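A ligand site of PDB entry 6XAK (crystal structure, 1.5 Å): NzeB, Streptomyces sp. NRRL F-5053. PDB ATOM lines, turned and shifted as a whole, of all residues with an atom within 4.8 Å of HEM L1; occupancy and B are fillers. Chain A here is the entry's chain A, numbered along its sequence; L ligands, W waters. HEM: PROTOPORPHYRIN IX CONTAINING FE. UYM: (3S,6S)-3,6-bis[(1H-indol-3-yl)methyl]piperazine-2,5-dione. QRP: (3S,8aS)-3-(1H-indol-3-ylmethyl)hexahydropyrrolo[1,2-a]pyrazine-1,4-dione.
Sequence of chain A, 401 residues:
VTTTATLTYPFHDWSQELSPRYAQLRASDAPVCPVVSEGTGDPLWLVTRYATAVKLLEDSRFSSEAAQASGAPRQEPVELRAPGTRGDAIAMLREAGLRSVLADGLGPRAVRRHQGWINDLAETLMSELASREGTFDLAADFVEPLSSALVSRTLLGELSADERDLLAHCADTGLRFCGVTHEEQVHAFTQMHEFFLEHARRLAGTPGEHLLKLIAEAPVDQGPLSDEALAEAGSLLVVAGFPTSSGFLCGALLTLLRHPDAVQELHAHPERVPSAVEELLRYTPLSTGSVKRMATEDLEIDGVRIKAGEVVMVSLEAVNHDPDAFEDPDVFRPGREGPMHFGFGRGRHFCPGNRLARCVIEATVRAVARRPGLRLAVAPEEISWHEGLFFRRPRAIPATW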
ATOM      1  N   SER A  64       1.042  13.713  11.540  1.00  0.00           N
ATOM      2  CA  SER A  64       0.292  14.629  12.405  1.00  0.00           C
ATOM      3  C   SER A  64      -1.191  14.289  12.404  1.00  0.00           C
ATOM      4  O   SER A  64      -1.837  14.289  13.461  1.00  0.00           O
ATOM      5  CB  SER A  64       0.471  16.073  11.959  1.00  0.00           C
ATOM      6  OG  SER A  64      -0.257  16.930  12.833  1.00  0.00           O
ATOM      7  N   GLN A  68      -4.350  13.343  15.375  1.00  0.00           N
ATOM      8  CA  GLN A  68      -5.525  14.181  15.605  1.00  0.00           C
ATOM      9  C   GLN A  68      -6.834  13.397  15.577  1.00  0.00           C
ATOM     10  O   GLN A  68      -7.870  13.960  15.950  1.00  0.00           O
ATOM     11  CB  GLN A  68      -5.607  15.295  14.549  1.00  0.00           C
ATOM     12  CG  GLN A  68      -4.380  16.234  14.498  1.00  0.00           C
ATOM     13  CD  GLN A  68      -4.386  17.104  13.245  1.00  0.00           C
ATOM     14  OE1 GLN A  68      -5.450  17.492  12.749  1.00  0.00           O
ATOM     15  NE2 GLN A  68      -3.207  17.379  12.708  1.00  0.00           N
ATOM     16  N   ILE A  90      -7.979  20.898   7.269  1.00  0.00           N
ATOM     17  CA  ILE A  90      -6.967  20.949   6.214  1.00  0.00           C
ATOM     18  C   ILE A  90      -7.216  19.876   5.168  1.00  0.00           C
ATOM     19  O   ILE A  90      -7.113  20.139   3.959  1.00  0.00           O
ATOM     20  CB  ILE A  90      -5.550  20.875   6.812  1.00  0.00           C
ATOM     21  CG1 ILE A  90      -5.237  22.199   7.503  1.00  0.00           C
ATOM     22  CG2 ILE A  90      -4.524  20.603   5.725  1.00  0.00           C
ATOM     23  CD1 ILE A  90      -3.979  22.169   8.326  1.00  0.00           C
ATOM     24  N   LEU A 102      -5.031  28.178   1.756  1.00  0.00           N
ATOM     25  CA  LEU A 102      -4.383  28.601   2.989  1.00  0.00           C
ATOM     26  C   LEU A 102      -3.087  29.334   2.697  1.00  0.00           C
ATOM     27  O   LEU A 102      -2.884  30.472   3.143  1.00  0.00           O
ATOM     28  CB  LEU A 102      -4.100  27.395   3.890  1.00  0.00           C
ATOM     29  CG  LEU A 102      -5.268  26.772   4.642  1.00  0.00           C
ATOM     30  CD1 LEU A 102      -4.763  25.626   5.504  1.00  0.00           C
ATOM     31  CD2 LEU A 102      -5.987  27.814   5.487  1.00  0.00           C
ATOM     32  N   LEU A 106      -2.287  33.365   3.282  1.00  0.00           N
ATOM     33  CA  LEU A 106      -1.381  33.641   4.393  1.00  0.00           C
ATOM     34  C   LEU A 106       0.065  33.847   3.958  1.00  0.00           C
ATOM     35  O   LEU A 106       0.916  34.153   4.815  1.00  0.00           O
ATOM     36  CB  LEU A 106      -1.440  32.511   5.423  1.00  0.00           C
ATOM     37  CG  LEU A 106      -2.827  32.239   6.011  1.00  0.00           C
ATOM     38  CD1 LEU A 106      -2.832  30.927   6.756  1.00  0.00           C
ATOM     39  CD2 LEU A 106      -3.223  33.391   6.906  1.00  0.00           C
ATOM     40  N   LEU A 150      -6.851  41.747  12.842  1.00  0.00           N
ATOM     41  CA  LEU A 150      -6.242  40.655  12.074  1.00  0.00           C
ATOM     42  C   LEU A 150      -7.267  39.575  11.746  1.00  0.00           C
ATOM     43  O   LEU A 150      -7.411  39.157  10.602  1.00  0.00           O
ATOM     44  CB  LEU A 150      -5.074  40.062  12.855  1.00  0.00           C
ATOM     45  CG  LEU A 150      -4.063  39.217  12.062  1.00  0.00           C
ATOM     46  CD1 LEU A 150      -3.243  40.115  11.168  1.00  0.00           C
ATOM     47  CD2 LEU A 150      -3.155  38.421  12.977  1.00  0.00           C
ATOM     48  N   LEU A 155      -8.961  36.686   8.218  1.00  0.00           N
ATOM     49  CA  LEU A 155      -9.472  35.337   8.422  1.00  0.00           C
ATOM     50  C   LEU A 155     -10.968  35.217   8.190  1.00  0.00           C
ATOM     51  O   LEU A 155     -11.378  34.482   7.280  1.00  0.00           O
ATOM     52  CB  LEU A 155      -9.101  34.825   9.822  1.00  0.00           C
ATOM     53  CG  LEU A 155      -7.617  34.919  10.151  1.00  0.00           C
ATOM     54  CD1 LEU A 155      -7.340  34.345  11.539  1.00  0.00           C
ATOM     55  CD2 LEU A 155      -6.824  34.204   9.080  1.00  0.00           C
ATOM     56  N   LEU A 236     -11.221  26.020  12.045  1.00  0.00           N
ATOM     57  CA  LEU A 236      -9.764  25.971  11.893  1.00  0.00           C
ATOM     58  C   LEU A 236      -9.142  27.356  12.062  1.00  0.00           C
ATOM     59  O   LEU A 236      -8.153  27.519  12.792  1.00  0.00           O
ATOM     60  CB  LEU A 236      -9.419  25.415  10.514  1.00  0.00           C
ATOM     61  CG  LEU A 236      -7.938  25.559  10.146  1.00  0.00           C
ATOM     62  CD1 LEU A 236      -7.103  24.726  11.104  1.00  0.00           C
ATOM     63  CD2 LEU A 236      -7.709  25.111   8.716  1.00  0.00           C
ATOM     64  N   LEU A 237      -9.711  28.371  11.405  1.00  0.00           N
ATOM     65  CA  LEU A 237      -9.149  29.710  11.465  1.00  0.00           C
ATOM     66  C   LEU A 237      -9.202  30.281  12.876  1.00  0.00           C
ATOM     67  O   LEU A 237      -8.291  31.017  13.283  1.00  0.00           O
ATOM     68  CB  LEU A 237      -9.877  30.618  10.478  1.00  0.00           C
ATOM     69  CG  LEU A 237      -9.766  30.158   9.016  1.00  0.00           C
ATOM     70  CD1 LEU A 237     -10.646  30.994   8.095  1.00  0.00           C
ATOM     71  CD2 LEU A 237      -8.339  30.207   8.559  1.00  0.00           C
ATOM     72  N   ALA A 240      -6.569  28.080  15.159  1.00  0.00           N
ATOM     73  CA  ALA A 240      -5.184  28.221  14.712  1.00  0.00           C
ATOM     74  C   ALA A 240      -4.704  29.666  14.706  1.00  0.00           C
ATOM     75  O   ALA A 240      -3.493  29.905  14.824  1.00  0.00           O
ATOM     76  CB  ALA A 240      -5.044  27.601  13.321  1.00  0.00           C
ATOM     77  N   GLY A 241      -5.609  30.642  14.559  1.00  0.00           N
ATOM     78  CA  GLY A 241      -5.182  32.017  14.403  1.00  0.00           C
ATOM     79  C   GLY A 241      -5.539  32.960  15.531  1.00  0.00           C
ATOM     80  O   GLY A 241      -4.899  34.013  15.681  1.00  0.00           O
ATOM     81  N   THR A 244      -3.379  31.852  19.288  1.00  0.00           N
ATOM     82  CA  THR A 244      -1.964  31.925  18.979  1.00  0.00           C
ATOM     83  C   THR A 244      -1.517  33.368  18.828  1.00  0.00           C
ATOM     84  O   THR A 244      -0.550  33.802  19.465  1.00  0.00           O
ATOM     85  CB  THR A 244      -1.728  31.168  17.677  1.00  0.00           C
ATOM     86  OG1 THR A 244      -2.676  31.640  16.708  1.00  0.00           O
ATOM     87  CG2 THR A 244      -1.948  29.669  17.868  1.00  0.00           C
ATOM     88  N   SER A 245      -2.222  34.143  18.003  1.00  0.00           N
ATOM     89  CA  SER A 245      -1.824  35.524  17.790  1.00  0.00           C
ATOM     90  C   SER A 245      -1.958  36.368  19.052  1.00  0.00           C
ATOM     91  O   SER A 245      -1.036  37.108  19.408  1.00  0.00           O
ATOM     92  CB  SER A 245      -2.621  36.128  16.623  1.00  0.00           C
ATOM     93  OG  SER A 245      -2.362  35.395  15.441  1.00  0.00           O
ATOM     94  N   PHE A 248       0.712  35.119  21.609  1.00  0.00           N
ATOM     95  CA  PHE A 248       2.105  35.402  21.289  1.00  0.00           C
ATOM     96  C   PHE A 248       2.416  36.873  21.388  1.00  0.00           C
ATOM     97  O   PHE A 248       3.468  37.261  21.902  1.00  0.00           O
ATOM     98  CB  PHE A 248       2.531  34.875  19.930  1.00  0.00           C
ATOM     99  CG  PHE A 248       3.997  35.012  19.734  1.00  0.00           C
ATOM    100  CD1 PHE A 248       4.866  34.099  20.303  1.00  0.00           C
ATOM    101  CD2 PHE A 248       4.528  36.131  19.097  1.00  0.00           C
ATOM    102  CE1 PHE A 248       6.247  34.244  20.187  1.00  0.00           C
ATOM    103  CE2 PHE A 248       5.900  36.296  18.971  1.00  0.00           C
ATOM    104  CZ  PHE A 248       6.771  35.350  19.534  1.00  0.00           C
ATOM    105  N   LEU A 281      10.393  34.733  18.584  1.00  0.00           N
ATOM    106  CA  LEU A 281       9.796  33.435  18.266  1.00  0.00           C
ATOM    107  C   LEU A 281      10.556  32.271  18.924  1.00  0.00           C
ATOM    108  O   LEU A 281       9.957  31.237  19.224  1.00  0.00           O
ATOM    109  CB  LEU A 281       9.735  33.248  16.755  1.00  0.00           C
ATOM    110  CG  LEU A 281       8.711  34.158  16.063  1.00  0.00           C
ATOM    111  CD1 LEU A 281       8.976  34.306  14.580  1.00  0.00           C
ATOM    112  CD2 LEU A 281       7.332  33.518  16.293  1.00  0.00           C
ATOM    113  N   LEU A 286       5.001  29.904  24.034  1.00  0.00           N
ATOM    114  CA  LEU A 286       3.608  30.041  23.664  1.00  0.00           C
ATOM    115  C   LEU A 286       2.791  28.851  24.157  1.00  0.00           C
ATOM    116  O   LEU A 286       2.114  28.930  25.194  1.00  0.00           O
ATOM    117  CB  LEU A 286       3.447  30.237  22.160  1.00  0.00           C
ATOM    118  CG  LEU A 286       2.019  30.540  21.670  1.00  0.00           C
ATOM    119  CD1 LEU A 286       1.372  31.779  22.351  1.00  0.00           C
ATOM    120  CD2 LEU A 286       2.032  30.683  20.157  1.00  0.00           C
ATOM    121  N   VAL A 291       3.648  19.927  20.076  1.00  0.00           N
ATOM    122  CA  VAL A 291       3.302  19.357  18.780  1.00  0.00           C
ATOM    123  C   VAL A 291       3.426  17.838  18.917  1.00  0.00           C
ATOM    124  O   VAL A 291       4.153  17.336  19.772  1.00  0.00           O
ATOM    125  CB  VAL A 291       4.193  19.879  17.635  1.00  0.00           C
ATOM    126  CG1 VAL A 291       4.129  21.407  17.564  1.00  0.00           C
ATOM    127  CG2 VAL A 291       5.599  19.398  17.782  1.00  0.00           C
ATOM    128  N   ARG A 293       2.921  13.713  16.875  1.00  0.00           N
ATOM    129  CA  ARG A 293       2.834  12.914  15.651  1.00  0.00           C
ATOM    130  C   ARG A 293       2.664  11.461  16.052  1.00  0.00           C
ATOM    131  O   ARG A 293       3.259  11.001  17.030  1.00  0.00           O
ATOM    132  CB  ARG A 293       4.131  13.018  14.836  1.00  0.00           C
ATOM    133  CG  ARG A 293       4.590  14.434  14.551  1.00  0.00           C
ATOM    134  CD  ARG A 293       3.695  15.077  13.507  1.00  0.00           C
ATOM    135  NE  ARG A 293       4.199  16.369  13.032  1.00  0.00           N
ATOM    136  CZ  ARG A 293       3.769  17.569  13.454  1.00  0.00           C
ATOM    137  NH1 ARG A 293       2.830  17.660  14.399  1.00  0.00           N
ATOM    138  NH2 ARG A 293       4.273  18.672  12.936  1.00  0.00           N
ATOM    139  N   LEU A 316       8.008  22.586  21.807  1.00  0.00           N
ATOM    140  CA  LEU A 316       8.779  23.579  21.060  1.00  0.00           C
ATOM    141  C   LEU A 316       9.542  24.491  22.003  1.00  0.00           C
ATOM    142  O   LEU A 316      10.664  24.940  21.665  1.00  0.00           O
ATOM    143  CB  LEU A 316       7.828  24.402  20.186  1.00  0.00           C
ATOM    144  CG  LEU A 316       6.966  23.591  19.218  1.00  0.00           C
ATOM    145  CD1 LEU A 316       6.109  24.602  18.416  1.00  0.00           C
ATOM    146  CD2 LEU A 316       7.816  22.740  18.295  1.00  0.00           C
ATOM    147  N   PHE A 342      12.239  26.856  16.545  1.00  0.00           N
ATOM    148  CA  PHE A 342      11.111  25.946  16.429  1.00  0.00           C
ATOM    149  C   PHE A 342       9.793  26.642  16.747  1.00  0.00           C
ATOM    150  O   PHE A 342       8.790  25.949  16.946  1.00  0.00           O
ATOM    151  CB  PHE A 342      11.292  24.757  17.370  1.00  0.00           C
ATOM    152  CG  PHE A 342      11.989  23.592  16.746  1.00  0.00           C
ATOM    153  CD1 PHE A 342      13.328  23.661  16.422  1.00  0.00           C
ATOM    154  CD2 PHE A 342      11.301  22.395  16.490  1.00  0.00           C
ATOM    155  CE1 PHE A 342      14.006  22.564  15.876  1.00  0.00           C
ATOM    156  CE2 PHE A 342      11.977  21.287  15.935  1.00  0.00           C
ATOM    157  CZ  PHE A 342      13.318  21.377  15.629  1.00  0.00           C
ATOM    158  N   GLY A 343       9.772  27.974  16.798  1.00  0.00           N
ATOM    159  CA  GLY A 343       8.549  28.672  17.196  1.00  0.00           C
ATOM    160  C   GLY A 343       7.379  28.439  16.252  1.00  0.00           C
ATOM    161  O   GLY A 343       6.232  28.552  16.661  1.00  0.00           O
ATOM    162  N   PHE A 344       7.657  28.126  14.983  1.00  0.00           N
ATOM    163  CA  PHE A 344       6.656  27.811  13.987  1.00  0.00           C
ATOM    164  C   PHE A 344       6.645  26.317  13.661  1.00  0.00           C
ATOM    165  O   PHE A 344       5.982  25.905  12.690  1.00  0.00           O
ATOM    166  CB  PHE A 344       6.912  28.588  12.703  1.00  0.00           C
ATOM    167  CG  PHE A 344       6.563  30.048  12.778  1.00  0.00           C
ATOM    168  CD1 PHE A 344       5.313  30.459  13.207  1.00  0.00           C
ATOM    169  CD2 PHE A 344       7.494  31.002  12.398  1.00  0.00           C
ATOM    170  CE1 PHE A 344       4.983  31.828  13.265  1.00  0.00           C
ATOM    171  CE2 PHE A 344       7.175  32.367  12.448  1.00  0.00           C
ATOM    172  CZ  PHE A 344       5.926  32.788  12.887  1.00  0.00           C
ATOM    173  N   GLY A 345       7.388  25.529  14.419  1.00  0.00           N
ATOM    174  CA  GLY A 345       7.534  24.109  14.157  1.00  0.00           C
ATOM    175  C   GLY A 345       8.639  23.804  13.171  1.00  0.00           C
ATOM    176  O   GLY A 345       9.610  24.557  13.048  1.00  0.00           O
ATOM    177  N   HIS A 349       4.556  20.461   8.461  1.00  0.00           N
ATOM    178  CA  HIS A 349       3.467  21.212   9.092  1.00  0.00           C
ATOM    179  C   HIS A 349       3.907  22.565   9.644  1.00  0.00           C
ATOM    180  O   HIS A 349       3.181  23.157  10.454  1.00  0.00           O
ATOM    181  CB  HIS A 349       2.798  20.373  10.178  1.00  0.00           C
ATOM    182  CG  HIS A 349       2.210  19.098   9.647  1.00  0.00           C
ATOM    183  ND1 HIS A 349       0.953  19.046   9.083  1.00  0.00           N
ATOM    184  CD2 HIS A 349       2.723  17.844   9.568  1.00  0.00           C
ATOM    185  CE1 HIS A 349       0.710  17.805   8.696  1.00  0.00           C
ATOM    186  NE2 HIS A 349       1.761  17.057   8.979  1.00  0.00           N
ATOM    187  N   CYS A 351       4.215  26.242  10.356  1.00  0.00           N
ATOM    188  CA  CYS A 351       3.051  27.110  10.397  1.00  0.00           C
ATOM    189  C   CYS A 351       2.762  27.761   9.052  1.00  0.00           C
ATOM    190  O   CYS A 351       3.558  28.579   8.568  1.00  0.00           O
ATOM    191  CB  CYS A 351       3.222  28.206  11.462  1.00  0.00           C
ATOM    192  SG  CYS A 351       1.901  29.436  11.392  1.00  0.00           S
ATOM    193  N   PRO A 352       1.627  27.433   8.406  1.00  0.00           N
ATOM    194  CA  PRO A 352       1.300  28.096   7.129  1.00  0.00           C
ATOM    195  C   PRO A 352       1.025  29.569   7.285  1.00  0.00           C
ATOM    196  O   PRO A 352       1.085  30.312   6.289  1.00  0.00           O
ATOM    197  CB  PRO A 352       0.052  27.330   6.637  1.00  0.00           C
ATOM    198  CG  PRO A 352      -0.481  26.636   7.837  1.00  0.00           C
ATOM    199  CD  PRO A 352       0.661  26.383   8.761  1.00  0.00           C
ATOM    200  N   GLY A 353       0.728  30.035   8.489  1.00  0.00           N
ATOM    201  CA  GLY A 353       0.552  31.443   8.727  1.00  0.00           C
ATOM    202  C   GLY A 353       1.823  32.181   9.127  1.00  0.00           C
ATOM    203  O   GLY A 353       1.740  33.302   9.627  1.00  0.00           O
ATOM    204  N   ALA A 357       2.064  35.983  10.640  1.00  0.00           N
ATOM    205  CA  ALA A 357       2.445  36.148  12.039  1.00  0.00           C
ATOM    206  C   ALA A 357       3.702  37.014  12.154  1.00  0.00           C
ATOM    207  O   ALA A 357       3.761  37.944  12.970  1.00  0.00           O
ATOM    208  CB  ALA A 357       2.687  34.782  12.687  1.00  0.00           C
ATOM    209  N   ILE A 361       3.933  40.478  14.264  1.00  0.00           N
ATOM    210  CA  ILE A 361       4.950  40.620  15.307  1.00  0.00           C
ATOM    211  C   ILE A 361       5.910  41.764  14.985  1.00  0.00           C
ATOM    212  O   ILE A 361       6.267  42.546  15.860  1.00  0.00           O
ATOM    213  CB  ILE A 361       5.728  39.293  15.531  1.00  0.00           C
ATOM    214  CG1 ILE A 361       4.775  38.153  15.911  1.00  0.00           C
ATOM    215  CG2 ILE A 361       6.841  39.461  16.592  1.00  0.00           C
ATOM    216  CD1 ILE A 361       5.395  36.762  15.648  1.00  0.00           C
HETATM  217  CHA HEM L   1       0.487  25.394  12.568  1.00  0.00           C
HETATM  218  CHB HEM L   1       2.793  28.558  15.443  1.00  0.00           C
HETATM  219  CHC HEM L   1      -0.198  32.096  13.975  1.00  0.00           C
HETATM  220  CHD HEM L   1      -2.414  28.919  11.003  1.00  0.00           C
HETATM  221  C1A HEM L   1       1.387  25.953  13.451  1.00  0.00           C
HETATM  222  C2A HEM L   1       2.457  25.247  14.117  1.00  0.00           C
HETATM  223  C3A HEM L   1       3.083  26.112  14.908  1.00  0.00           C
HETATM  224  C4A HEM L   1       2.432  27.408  14.786  1.00  0.00           C
HETATM  225  CMA HEM L   1       4.290  25.773  15.802  1.00  0.00           C
HETATM  226  CAA HEM L   1       2.889  23.771  13.938  1.00  0.00           C
HETATM  227  CBA HEM L   1       1.986  22.751  14.629  1.00  0.00           C
HETATM  228  CGA HEM L   1       2.476  21.340  14.398  1.00  0.00           C
HETATM  229  O1A HEM L   1       3.627  21.124  13.933  1.00  0.00           O
HETATM  230  O2A HEM L   1       1.700  20.387  14.678  1.00  0.00           O
HETATM  231  C1B HEM L   1       2.179  29.787  15.295  1.00  0.00           C
HETATM  232  C2B HEM L   1       2.589  31.004  15.986  1.00  0.00           C
HETATM  233  C3B HEM L   1       1.732  31.984  15.589  1.00  0.00           C
HETATM  234  C4B HEM L   1       0.810  31.406  14.622  1.00  0.00           C
HETATM  235  CMB HEM L   1       3.755  31.036  17.001  1.00  0.00           C
HETATM  236  CAB HEM L   1       1.709  33.479  15.994  1.00  0.00           C
HETATM  237  CBB HEM L   1       2.753  34.082  16.577  1.00  0.00           C
HETATM  238  C1C HEM L   1      -1.059  31.535  13.033  1.00  0.00           C
HETATM  239  C2C HEM L   1      -2.095  32.245  12.325  1.00  0.00           C
HETATM  240  C3C HEM L   1      -2.721  31.380  11.534  1.00  0.00           C
HETATM  241  C4C HEM L   1      -2.093  30.078  11.676  1.00  0.00           C
HETATM  242  CMC HEM L   1      -2.401  33.741  12.515  1.00  0.00           C
HETATM  243  CAC HEM L   1      -3.899  31.763  10.606  1.00  0.00           C
HETATM  244  CBC HEM L   1      -4.936  30.955  10.401  1.00  0.00           C
HETATM  245  C1D HEM L   1      -1.895  27.668  11.234  1.00  0.00           C
HETATM  246  C2D HEM L   1      -2.439  26.407  10.757  1.00  0.00           C
HETATM  247  C3D HEM L   1      -1.645  25.416  11.210  1.00  0.00           C
HETATM  248  C4D HEM L   1      -0.572  26.037  11.962  1.00  0.00           C
HETATM  249  CMD HEM L   1      -3.728  26.239   9.918  1.00  0.00           C
HETATM  250  CAD HEM L   1      -1.798  23.877  11.012  1.00  0.00           C
HETATM  251  CBD HEM L   1      -0.954  23.353   9.876  1.00  0.00           C
HETATM  252  CGD HEM L   1      -0.861  21.840   9.892  1.00  0.00           C
HETATM  253  O1D HEM L   1      -1.285  21.168  10.865  1.00  0.00           O
HETATM  254  O2D HEM L   1      -0.355  21.291   8.881  1.00  0.00           O
HETATM  255  NA  HEM L   1       1.395  27.264  13.880  1.00  0.00           N
HETATM  256  NB  HEM L   1       1.083  30.057  14.474  1.00  0.00           N
HETATM  257  NC  HEM L   1      -1.068  30.213  12.595  1.00  0.00           N
HETATM  258  ND  HEM L   1      -0.748  27.398  11.961  1.00  0.00           N
HETATM  259 FE   HEM L   1       0.350  28.803  13.041  1.00  0.00          FE
HETATM  260  N   UYM L   2      -9.034  21.348  16.436  1.00  0.00           N
HETATM  261  C   UYM L   2      -4.568  21.479  12.765  1.00  0.00           C
HETATM  262  O   UYM L   2      -4.799  22.075  11.755  1.00  0.00           O
HETATM  263  C1  UYM L   2      -5.748  21.076  13.666  1.00  0.00           C
HETATM  264  C10 UYM L   2     -11.353  21.729  15.204  1.00  0.00           C
HETATM  265  C11 UYM L   2      -2.776  20.427  14.301  1.00  0.00           C
HETATM  266  C12 UYM L   2      -1.906  21.304  15.245  1.00  0.00           C
HETATM  267  C15 UYM L   2      -3.964  19.920  15.118  1.00  0.00           C
HETATM  268  C2  UYM L   2      -6.460  22.333  14.185  1.00  0.00           C
HETATM  269  C3  UYM L   2      -7.799  21.987  14.939  1.00  0.00           C
HETATM  270  C34 UYM L   2      -2.516  22.716  15.613  1.00  0.00           C
HETATM  271  C35 UYM L   2      -2.237  23.684  14.854  1.00  0.00           C
HETATM  272  C37 UYM L   2      -3.574  24.294  16.610  1.00  0.00           C
HETATM  273  C38 UYM L   2      -3.246  22.944  16.627  1.00  0.00           C
HETATM  274  C39 UYM L   2      -3.732  22.131  17.675  1.00  0.00           C
HETATM  275  C4  UYM L   2      -7.759  21.513  16.152  1.00  0.00           C
HETATM  276  C40 UYM L   2      -4.563  22.689  18.672  1.00  0.00           C
HETATM  277  C41 UYM L   2      -4.879  24.048  18.642  1.00  0.00           C
HETATM  278  C42 UYM L   2      -4.392  24.855  17.622  1.00  0.00           C
HETATM  279  C5  UYM L   2      -9.973  21.706  15.424  1.00  0.00           C
HETATM  280  C6  UYM L   2      -9.054  22.139  14.398  1.00  0.00           C
HETATM  281  C7  UYM L   2      -9.598  22.578  13.186  1.00  0.00           C
HETATM  282  C8  UYM L   2     -10.985  22.600  12.958  1.00  0.00           C
HETATM  283  C9  UYM L   2     -11.874  22.174  13.971  1.00  0.00           C
HETATM  284  N1  UYM L   2      -5.327  20.253  14.777  1.00  0.00           N
HETATM  285  N2  UYM L   2      -3.200  21.135  13.118  1.00  0.00           N
HETATM  286  N36 UYM L   2      -2.893  24.819  15.385  1.00  0.00           N
HETATM  287  O1  UYM L   2      -3.753  19.223  16.051  1.00  0.00           O
HETATM  288  C   QRP L   3      -1.245  20.869  19.647  1.00  0.00           C
HETATM  289  N   QRP L   3      -0.351  22.773  20.922  1.00  0.00           N
HETATM  290  O   QRP L   3      -1.053  20.055  18.765  1.00  0.00           O
HETATM  291  CA  QRP L   3      -0.569  22.210  19.599  1.00  0.00           C
HETATM  292  CB  QRP L   3       0.762  22.149  18.840  1.00  0.00           C
HETATM  293  CG  QRP L   3       1.465  23.484  19.022  1.00  0.00           C
HETATM  294  OAA QRP L   3      -1.036  23.124  23.069  1.00  0.00           O
HETATM  295  CAH QRP L   3      -3.498  19.635  22.254  1.00  0.00           C
HETATM  296  CAI QRP L   3      -2.631  20.692  22.916  1.00  0.00           C
HETATM  297  CAJ QRP L   3      -2.858  19.403  20.879  1.00  0.00           C
HETATM  298  CAN QRP L   3      -1.172  22.574  21.978  1.00  0.00           C
HETATM  299  CAT QRP L   3      -2.300  21.595  21.734  1.00  0.00           C
HETATM  300  NAU QRP L   3      -2.083  20.634  20.659  1.00  0.00           N
HETATM  301  CD1 QRP L   3       2.587  23.674  19.807  1.00  0.00           C
HETATM  302  CD2 QRP L   3       1.137  24.735  18.489  1.00  0.00           C
HETATM  303  NE1 QRP L   3       2.968  24.983  19.746  1.00  0.00           N
HETATM  304  CE2 QRP L   3       2.098  25.635  18.969  1.00  0.00           C
HETATM  305  CE3 QRP L   3       0.116  25.154  17.646  1.00  0.00           C
HETATM  306  CH2 QRP L   3       1.019  27.397  17.770  1.00  0.00           C
HETATM  307  CZ2 QRP L   3       2.040  26.978  18.612  1.00  0.00           C
HETATM  308  CZ3 QRP L   3       0.063  26.491  17.273  1.00  0.00           C
HETATM  309  O   HOH W   1      -2.734  18.826  10.291  1.00  0.00           O
HETATM  310  O   HOH W   2       0.700  19.020  16.793  1.00  0.00           O
HETATM  311  O   HOH W   3       0.313  19.490  12.513  1.00  0.00           O
HETATM  312  O   HOH W   4      -0.037  22.714   6.625  1.00  0.00           O
HETATM  313  O   HOH W   5       5.638  21.958  12.315  1.00  0.00           O
HETATM  314  O   HOH W   6      -1.989  27.562  14.704  1.00  0.00           O
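An iron atom (FE) of HEM L1 is bound by the side-chain sulfur (SG) of Cys 351. A ring nitrogen (ND1) of His 349 is in hydrogen-bond range of an oxygen (O2D) of HEM L1, at 2.6 Å. The guanidinium group (NH2) of Arg 293 lies within salt-bridge range of an oxygen (O1A) of HEM L1 (2.7 Å). OE1 of Gln 68 lies within hydrogen-bond range of N1 of UYM L2, at 3.4 Å.
The backbone carbonyl oxygen of Ala 240 lies close to a nitrogen (NC) of HEM L1, 3.3 Å away. Merely in contact with HEM L1: Phe 344, Ser 245, Leu 316, Gly 345, Pro 352, Phe 248, Gly 343, Ile 90, Val 291, Leu 286, Ala 357, Thr 244, Gly 241, Ile 361, Leu 236, Leu 237 and Leu 155. Hydrophobic or aromatic side chains within 4 Å of HEM L1: Ile 90, Leu 155, Leu 236, Leu 237, Ala 240, Phe 248, Leu 286, Val 291, Leu 316, Phe 344, His 349, Pro 352, Ala 357 and Ile 361. Of the 29 residues printed, 21 come within 4 Å of HEM L1.
Water W2 lies within hydrogen-bond range of an oxygen (O2A) of HEM L1 (2.7 Å), an oxygen (O) of QRP L3 (2.8 Å) and the guanidinium group (NH1) of Arg 293 (3.5 Å). Water W5 lies within hydrogen-bond range of an oxygen (O1A) of HEM L1 and the backbone carbonyl oxygen (O) of His 349. Water W3 lies within hydrogen-bond range of the side-chain hydroxyl of Ser 64 (2.6 Å) and an oxygen (O2A) of HEM L1 (2.7 Å). Water W1 lies within hydrogen-bond range of an oxygen (O1D) of HEM L1 (2.8 Å) and the side-chain amide nitrogen of Gln 68 (2.9 Å). Water W6 bridges O of Ala 240 (2.8 Å) and N36 of UYM L2 (3.0 Å).
A nitrogen (N2) of UYM L2 sits at hydrogen-bond distance from an oxygen (O1D) of HEM L1, 3.0 Å away.
The backbone NH (N) of Cys 351 is in hydrogen-bond range of the backbone carbonyl oxygen (O) of Phe 344, at 2.9 Å. SG of Cys 351 lies close to N of Gly 353 (3.2 Å). The side-chain hydroxyl (OG1) of Thr 244 is in hydrogen-bond range of the backbone carbonyl oxygen (O) of Ala 240 (2.7 Å). The side-chain hydroxyl of Ser 245 sits at hydrogen-bond distance from the backbone carbonyl oxygen of Gly 241 (2.9 Å). The side-chain hydroxyl (OG1) of Thr 244 sits close to the backbone carbonyl oxygen (O) of Gly 241, at 3.4 Å.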
